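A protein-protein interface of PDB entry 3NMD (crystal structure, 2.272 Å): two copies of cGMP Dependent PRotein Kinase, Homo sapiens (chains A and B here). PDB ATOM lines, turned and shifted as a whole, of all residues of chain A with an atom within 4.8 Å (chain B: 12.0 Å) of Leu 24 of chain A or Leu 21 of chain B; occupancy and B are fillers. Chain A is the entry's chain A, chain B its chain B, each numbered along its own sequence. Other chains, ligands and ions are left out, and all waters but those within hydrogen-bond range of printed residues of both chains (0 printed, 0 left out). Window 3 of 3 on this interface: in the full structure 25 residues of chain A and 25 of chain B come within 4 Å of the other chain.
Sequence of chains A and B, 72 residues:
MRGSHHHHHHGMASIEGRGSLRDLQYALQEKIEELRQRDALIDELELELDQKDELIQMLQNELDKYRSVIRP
Hydrophobic or aromatic side chains of chain B within 4 Å of the printed part of chain A: Leu 21, Leu 24, Ala 27 and Leu 28.
Hydrophobic or aromatic side chains of chain A that line the printed part of chain B: Leu 21, Leu 24 and Leu 28.
Among the printed residues, 9 pairs touch across the chains.
Among the printed residues, no Asp or Glu carboxylate lies within 4 Å of a Lys or Arg side-chain nitrogen of the other chain.
Of the printed residues of chain A, Leu 21 of chain B touches Leu 24.
Of the printed residues of chain B, Leu 21 of chain A touches Leu 24.
No residue of chain B comes within 4 Å of Asp 23 of chain A.
Of chain B, only Leu 28 comes within 4 Å of Ala 27 of chain A.
Printed residues of chain A within 4 Å of Leu 28 of chain B: Leu 24, Ala 27 and Leu 28.
Printed residues of chain A within 4 Å of Leu 24 of chain B: Leu 21 and Gln 25.
Tyr 26 of chain A touches none of the printed residues of chain B.
The nearest residue of chain A that does not touch Leu 21 of chain B is Leu 21 of chain A (4.1 Å).
The nearest printed residue of chain A that does not touch Gln 25 of chain B is Leu 28 of chain A (6.7 Å).
Leu 21 of chain A touches Leu 24 of chain B, and with the chains exchanged Leu 24 of chain A touches Leu 21 of chain B.
Leu 24 of chain A touches Leu 28 of chain B, but with the chains exchanged Leu 28 of chain A does not touch Leu 24 of chain B (4.001 Å).
Ala 27 of chain A touches Leu 28 of chain B, and with the chains exchanged Leu 28 of chain A touches Ala 27 of chain B.
Leu 28 of chain B touches its own counterpart, Leu 28 of chain A.
Positions printed for both chains: 21, 22, 23, 24, 25, 26, 27 and 28.
Among the printed residues, merely in contact across the chains: Leu 21 of chain A with Leu 24 of chain B (3.3 Å), Leu 24 of chain A with Leu 21 of chain B (3.8 Å), Leu 24 of chain A with Gln 25 of chain B (3.98 Å), Leu 24 of chain A with Leu 28 of chain B (3.99 Å), Gln 25 of chain A with Leu 24 of chain B (3.9 Å), Ala 27 of chain A with Leu 28 of chain B (3.8 Å), Leu 28 of chain A with Ala 27 of chain B (3.7 Å), Leu 28 of chain A with Leu 28 of chain B (3.8 Å) and Leu 28 of chain A with Lys 31 of chain B (3.6 Å).
NH1 of Arg 22 of chain A is in hydrogen-bond range of OE1 of Gln 25 of chain A (2.8 Å).
The backbone carbonyl oxygen (O) of Leu 21 of chain B lies within hydrogen-bond range of the side-chain amide nitrogen (NE2) of Gln 25 of chain B (3.5 Å).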
ATOM      1  N   SER A  20      27.942  -0.182 -15.890  1.00  0.00           N
ATOM      2  CA  SER A  20      26.912   0.631 -16.516  1.00  0.00           C
ATOM      3  C   SER A  20      27.255   0.741 -17.999  1.00  0.00           C
ATOM      4  O   SER A  20      26.386   0.612 -18.855  1.00  0.00           O
ATOM      5  CB  SER A  20      26.836   2.010 -15.862  1.00  0.00           C
ATOM      6  OG  SER A  20      28.136   2.522 -15.625  1.00  0.00           O
ATOM      7  N   LEU A  21      28.538   0.956 -18.283  1.00  0.00           N
ATOM      8  CA  LEU A  21      29.053   0.951 -19.649  1.00  0.00           C
ATOM      9  C   LEU A  21      28.605  -0.293 -20.418  1.00  0.00           C
ATOM     10  O   LEU A  21      28.061  -0.186 -21.522  1.00  0.00           O
ATOM     11  CB  LEU A  21      30.582   1.041 -19.644  1.00  0.00           C
ATOM     12  CG  LEU A  21      31.255   0.888 -21.009  1.00  0.00           C
ATOM     13  CD1 LEU A  21      30.867   2.044 -21.912  1.00  0.00           C
ATOM     14  CD2 LEU A  21      32.774   0.798 -20.884  1.00  0.00           C
ATOM     15  N   ARG A  22      28.831  -1.470 -19.839  1.00  0.00           N
ATOM     16  CA  ARG A  22      28.439  -2.712 -20.500  1.00  0.00           C
ATOM     17  C   ARG A  22      26.934  -2.795 -20.742  1.00  0.00           C
ATOM     18  O   ARG A  22      26.502  -3.246 -21.805  1.00  0.00           O
ATOM     19  CB  ARG A  22      28.927  -3.927 -19.719  1.00  0.00           C
ATOM     20  CG  ARG A  22      30.442  -4.030 -19.660  1.00  0.00           C
ATOM     21  CD  ARG A  22      31.039  -4.565 -20.961  1.00  0.00           C
ATOM     22  NE  ARG A  22      32.466  -4.809 -20.755  1.00  0.00           N
ATOM     23  CZ  ARG A  22      33.433  -3.975 -21.127  1.00  0.00           C
ATOM     24  NH1 ARG A  22      33.135  -2.851 -21.767  1.00  0.00           N
ATOM     25  NH2 ARG A  22      34.695  -4.272 -20.871  1.00  0.00           N
ATOM     26  N   ASP A  23      26.145  -2.354 -19.761  1.00  0.00           N
ATOM     27  CA  ASP A  23      24.686  -2.335 -19.888  1.00  0.00           C
ATOM     28  C   ASP A  23      24.243  -1.493 -21.081  1.00  0.00           C
ATOM     29  O   ASP A  23      23.372  -1.897 -21.853  1.00  0.00           O
ATOM     30  CB  ASP A  23      24.042  -1.794 -18.612  1.00  0.00           C
ATOM     31  CG  ASP A  23      24.239  -2.717 -17.422  1.00  0.00           C
ATOM     32  OD1 ASP A  23      24.388  -3.941 -17.635  1.00  0.00           O
ATOM     33  OD2 ASP A  23      24.248  -2.217 -16.276  1.00  0.00           O
ATOM     34  N   LEU A  24      24.849  -0.317 -21.205  1.00  0.00           N
ATOM     35  CA  LEU A  24      24.615   0.585 -22.322  1.00  0.00           C
ATOM     36  C   LEU A  24      25.087  -0.007 -23.642  1.00  0.00           C
ATOM     37  O   LEU A  24      24.404   0.108 -24.655  1.00  0.00           O
ATOM     38  CB  LEU A  24      25.339   1.913 -22.092  1.00  0.00           C
ATOM     39  CG  LEU A  24      24.719   2.856 -21.060  1.00  0.00           C
ATOM     40  CD1 LEU A  24      25.592   4.089 -20.882  1.00  0.00           C
ATOM     41  CD2 LEU A  24      23.312   3.250 -21.469  1.00  0.00           C
ATOM     42  N   GLN A  25      26.266  -0.623 -23.634  1.00  0.00           N
ATOM     43  CA  GLN A  25      26.790  -1.203 -24.860  1.00  0.00           C
ATOM     44  C   GLN A  25      25.850  -2.296 -25.339  1.00  0.00           C
ATOM     45  O   GLN A  25      25.506  -2.336 -26.521  1.00  0.00           O
ATOM     46  CB  GLN A  25      28.211  -1.742 -24.670  1.00  0.00           C
ATOM     47  CG  GLN A  25      29.235  -0.648 -24.355  1.00  0.00           C
ATOM     48  CD  GLN A  25      30.619  -1.196 -24.046  1.00  0.00           C
ATOM     49  OE1 GLN A  25      30.798  -1.998 -23.122  1.00  0.00           O
ATOM     50  NE2 GLN A  25      31.606  -0.767 -24.821  1.00  0.00           N
ATOM     51  N   TYR A  26      25.425  -3.171 -24.425  1.00  0.00           N
ATOM     52  CA  TYR A  26      24.493  -4.225 -24.808  1.00  0.00           C
ATOM     53  C   TYR A  26      23.164  -3.667 -25.330  1.00  0.00           C
ATOM     54  O   TYR A  26      22.597  -4.181 -26.294  1.00  0.00           O
ATOM     55  CB  TYR A  26      24.208  -5.229 -23.681  1.00  0.00           C
ATOM     56  CG  TYR A  26      23.207  -6.252 -24.174  1.00  0.00           C
ATOM     57  CD1 TYR A  26      23.625  -7.339 -24.932  1.00  0.00           C
ATOM     58  CD2 TYR A  26      21.837  -6.087 -23.962  1.00  0.00           C
ATOM     59  CE1 TYR A  26      22.719  -8.262 -25.432  1.00  0.00           C
ATOM     60  CE2 TYR A  26      20.916  -7.009 -24.468  1.00  0.00           C
ATOM     61  CZ  TYR A  26      21.369  -8.095 -25.194  1.00  0.00           C
ATOM     62  OH  TYR A  26      20.488  -9.025 -25.701  1.00  0.00           O
ATOM     63  N   ALA A  27      22.655  -2.629 -24.678  1.00  0.00           N
ATOM     64  CA  ALA A  27      21.370  -2.054 -25.075  1.00  0.00           C
ATOM     65  C   ALA A  27      21.461  -1.443 -26.470  1.00  0.00           C
ATOM     66  O   ALA A  27      20.552  -1.596 -27.289  1.00  0.00           O
ATOM     67  CB  ALA A  27      20.903  -1.019 -24.053  1.00  0.00           C
ATOM     68  N   LEU A  28      22.573  -0.767 -26.742  1.00  0.00           N
ATOM     69  CA  LEU A  28      22.803  -0.175 -28.049  1.00  0.00           C
ATOM     70  C   LEU A  28      22.890  -1.273 -29.108  1.00  0.00           C
ATOM     71  O   LEU A  28      22.201  -1.232 -30.128  1.00  0.00           O
ATOM     72  CB  LEU A  28      24.093   0.661 -28.036  1.00  0.00           C
ATOM     73  CG  LEU A  28      24.378   1.505 -29.285  1.00  0.00           C
ATOM     74  CD1 LEU A  28      23.188   2.398 -29.641  1.00  0.00           C
ATOM     75  CD2 LEU A  28      25.644   2.332 -29.111  1.00  0.00           C
ATOM     76  N   LEU B  21      30.924   8.509 -22.153  1.00  0.00           N
ATOM     77  CA  LEU B  21      29.765   7.658 -21.911  1.00  0.00           C
ATOM     78  C   LEU B  21      28.443   8.356 -22.250  1.00  0.00           C
ATOM     79  O   LEU B  21      27.409   7.705 -22.416  1.00  0.00           O
ATOM     80  CB  LEU B  21      29.762   7.166 -20.466  1.00  0.00           C
ATOM     81  CG  LEU B  21      28.635   6.208 -20.082  1.00  0.00           C
ATOM     82  CD1 LEU B  21      29.181   4.994 -19.352  1.00  0.00           C
ATOM     83  CD2 LEU B  21      27.576   6.921 -19.256  1.00  0.00           C
ATOM     84  N   ARG B  22      28.477   9.681 -22.350  1.00  0.00           N
ATOM     85  CA  ARG B  22      27.314  10.420 -22.826  1.00  0.00           C
ATOM     86  C   ARG B  22      27.089  10.142 -24.307  1.00  0.00           C
ATOM     87  O   ARG B  22      25.954  10.135 -24.776  1.00  0.00           O
ATOM     88  CB  ARG B  22      27.451  11.923 -22.569  1.00  0.00           C
ATOM     89  CG  ARG B  22      26.822  12.369 -21.258  1.00  0.00           C
ATOM     90  N   ASP B  23      28.173   9.890 -25.035  1.00  0.00           N
ATOM     91  CA  ASP B  23      28.077   9.545 -26.449  1.00  0.00           C
ATOM     92  C   ASP B  23      27.234   8.284 -26.659  1.00  0.00           C
ATOM     93  O   ASP B  23      26.464   8.195 -27.620  1.00  0.00           O
ATOM     94  CB  ASP B  23      29.471   9.369 -27.060  1.00  0.00           C
ATOM     95  N   LEU B  24      27.388   7.318 -25.755  1.00  0.00           N
ATOM     96  CA  LEU B  24      26.627   6.071 -25.792  1.00  0.00           C
ATOM     97  C   LEU B  24      25.153   6.290 -25.463  1.00  0.00           C
ATOM     98  O   LEU B  24      24.279   5.718 -26.106  1.00  0.00           O
ATOM     99  CB  LEU B  24      27.208   5.049 -24.809  1.00  0.00           C
ATOM    100  CG  LEU B  24      28.501   4.339 -25.201  1.00  0.00           C
ATOM    101  CD1 LEU B  24      28.788   3.221 -24.211  1.00  0.00           C
ATOM    102  CD2 LEU B  24      28.415   3.799 -26.626  1.00  0.00           C
ATOM    103  N   GLN B  25      24.882   7.104 -24.448  1.00  0.00           N
ATOM    104  CA  GLN B  25      23.503   7.458 -24.113  1.00  0.00           C
ATOM    105  C   GLN B  25      22.787   8.180 -25.262  1.00  0.00           C
ATOM    106  O   GLN B  25      21.633   7.873 -25.573  1.00  0.00           O
ATOM    107  CB  GLN B  25      23.455   8.305 -22.847  1.00  0.00           C
ATOM    108  CG  GLN B  25      23.703   7.525 -21.568  1.00  0.00           C
ATOM    109  CD  GLN B  25      23.925   8.433 -20.368  1.00  0.00           C
ATOM    110  OE1 GLN B  25      23.111   8.470 -19.446  1.00  0.00           O
ATOM    111  NE2 GLN B  25      25.026   9.183 -20.383  1.00  0.00           N
ATOM    112  N   TYR B  26      23.467   9.135 -25.892  1.00  0.00           N
ATOM    113  CA  TYR B  26      22.885   9.841 -27.034  1.00  0.00           C
ATOM    114  C   TYR B  26      22.669   8.890 -28.207  1.00  0.00           C
ATOM    115  O   TYR B  26      21.651   8.961 -28.888  1.00  0.00           O
ATOM    116  CB  TYR B  26      23.746  11.039 -27.457  1.00  0.00           C
ATOM    117  CG  TYR B  26      23.612  12.249 -26.546  1.00  0.00           C
ATOM    118  CD1 TYR B  26      22.485  13.065 -26.596  1.00  0.00           C
ATOM    119  CD2 TYR B  26      24.616  12.575 -25.635  1.00  0.00           C
ATOM    120  CE1 TYR B  26      22.362  14.173 -25.762  1.00  0.00           C
ATOM    121  CE2 TYR B  26      24.503  13.676 -24.800  1.00  0.00           C
ATOM    122  CZ  TYR B  26      23.375  14.472 -24.865  1.00  0.00           C
ATOM    123  OH  TYR B  26      23.265  15.564 -24.031  1.00  0.00           O
ATOM    124  N   ALA B  27      23.633   7.998 -28.429  1.00  0.00           N
ATOM    125  CA  ALA B  27      23.537   6.993 -29.480  1.00  0.00           C
ATOM    126  C   ALA B  27      22.349   6.065 -29.241  1.00  0.00           C
ATOM    127  O   ALA B  27      21.614   5.726 -30.169  1.00  0.00           O
ATOM    128  CB  ALA B  27      24.835   6.182 -29.553  1.00  0.00           C
ATOM    129  N   LEU B  28      22.173   5.651 -27.990  1.00  0.00           N
ATOM    130  CA  LEU B  28      21.084   4.761 -27.614  1.00  0.00           C
ATOM    131  C   LEU B  28      19.747   5.460 -27.793  1.00  0.00           C
ATOM    132  O   LEU B  28      18.797   4.883 -28.320  1.00  0.00           O
ATOM    133  CB  LEU B  28      21.244   4.302 -26.160  1.00  0.00           C
ATOM    134  CG  LEU B  28      20.141   3.385 -25.630  1.00  0.00           C
ATOM    135  CD1 LEU B  28      20.059   2.100 -26.459  1.00  0.00           C
ATOM    136  CD2 LEU B  28      20.378   3.070 -24.164  1.00  0.00           C
ATOM    137  N   GLN B  29      19.683   6.716 -27.373  1.00  0.00           N
ATOM    138  CA  GLN B  29      18.456   7.488 -27.504  1.00  0.00           C
ATOM    139  C   GLN B  29      18.042   7.633 -28.965  1.00  0.00           C
ATOM    140  O   GLN B  29      16.860   7.531 -29.299  1.00  0.00           O
ATOM    141  CB  GLN B  29      18.605   8.859 -26.845  1.00  0.00           C
ATOM    142  CG  GLN B  29      17.286   9.599 -26.704  1.00  0.00           C
ATOM    143  CD  GLN B  29      16.222   8.761 -26.011  1.00  0.00           C
ATOM    144  OE1 GLN B  29      15.071   8.698 -26.455  1.00  0.00           O
ATOM    145  NE2 GLN B  29      16.608   8.105 -24.922  1.00  0.00           N
ATOM    146  N   GLU B  30      19.018   7.862 -29.834  1.00  0.00           N
ATOM    147  CA  GLU B  30      18.746   7.993 -31.262  1.00  0.00           C
ATOM    148  C   GLU B  30      18.197   6.682 -31.846  1.00  0.00           C
ATOM    149  O   GLU B  30      17.252   6.691 -32.630  1.00  0.00           O
ATOM    150  CB  GLU B  30      20.014   8.428 -31.999  1.00  0.00           C
ATOM    151  CG  GLU B  30      19.789   8.825 -33.450  1.00  0.00           C
ATOM    152  CD  GLU B  30      21.086   9.003 -34.215  1.00  0.00           C
ATOM    153  OE1 GLU B  30      21.112   9.828 -35.152  1.00  0.00           O
ATOM    154  OE2 GLU B  30      22.076   8.320 -33.878  1.00  0.00           O
ATOM    155  N   LYS B  31      18.789   5.556 -31.453  1.00  0.00           N
ATOM    156  CA  LYS B  31      18.330   4.249 -31.920  1.00  0.00           C
ATOM    157  C   LYS B  31      16.920   3.937 -31.418  1.00  0.00           C
ATOM    158  O   LYS B  31      16.128   3.325 -32.121  1.00  0.00           O
ATOM    159  CB  LYS B  31      19.301   3.142 -31.495  1.00  0.00           C
ATOM    160  CG  LYS B  31      20.686   3.238 -32.133  1.00  0.00           C
ATOM    161  CD  LYS B  31      20.561   3.460 -33.625  1.00  0.00           C
ATOM    162  CE  LYS B  31      21.910   3.531 -34.311  1.00  0.00           C
ATOM    163  NZ  LYS B  31      21.776   4.132 -35.673  1.00  0.00           N
ATOM    164  N   ILE B  32      16.616   4.357 -30.196  1.00  0.00           N
ATOM    165  CA  ILE B  32      15.275   4.195 -29.658  1.00  0.00           C
ATOM    166  C   ILE B  32      14.252   4.941 -30.525  1.00  0.00           C
ATOM    167  O   ILE B  32      13.228   4.381 -30.928  1.00  0.00           O
ATOM    168  CB  ILE B  32      15.201   4.664 -28.178  1.00  0.00           C
ATOM    169  CG1 ILE B  32      15.943   3.681 -27.270  1.00  0.00           C
ATOM    170  CG2 ILE B  32      13.753   4.802 -27.711  1.00  0.00           C
ATOM    171  CD1 ILE B  32      16.216   4.223 -25.867  1.00  0.00           C
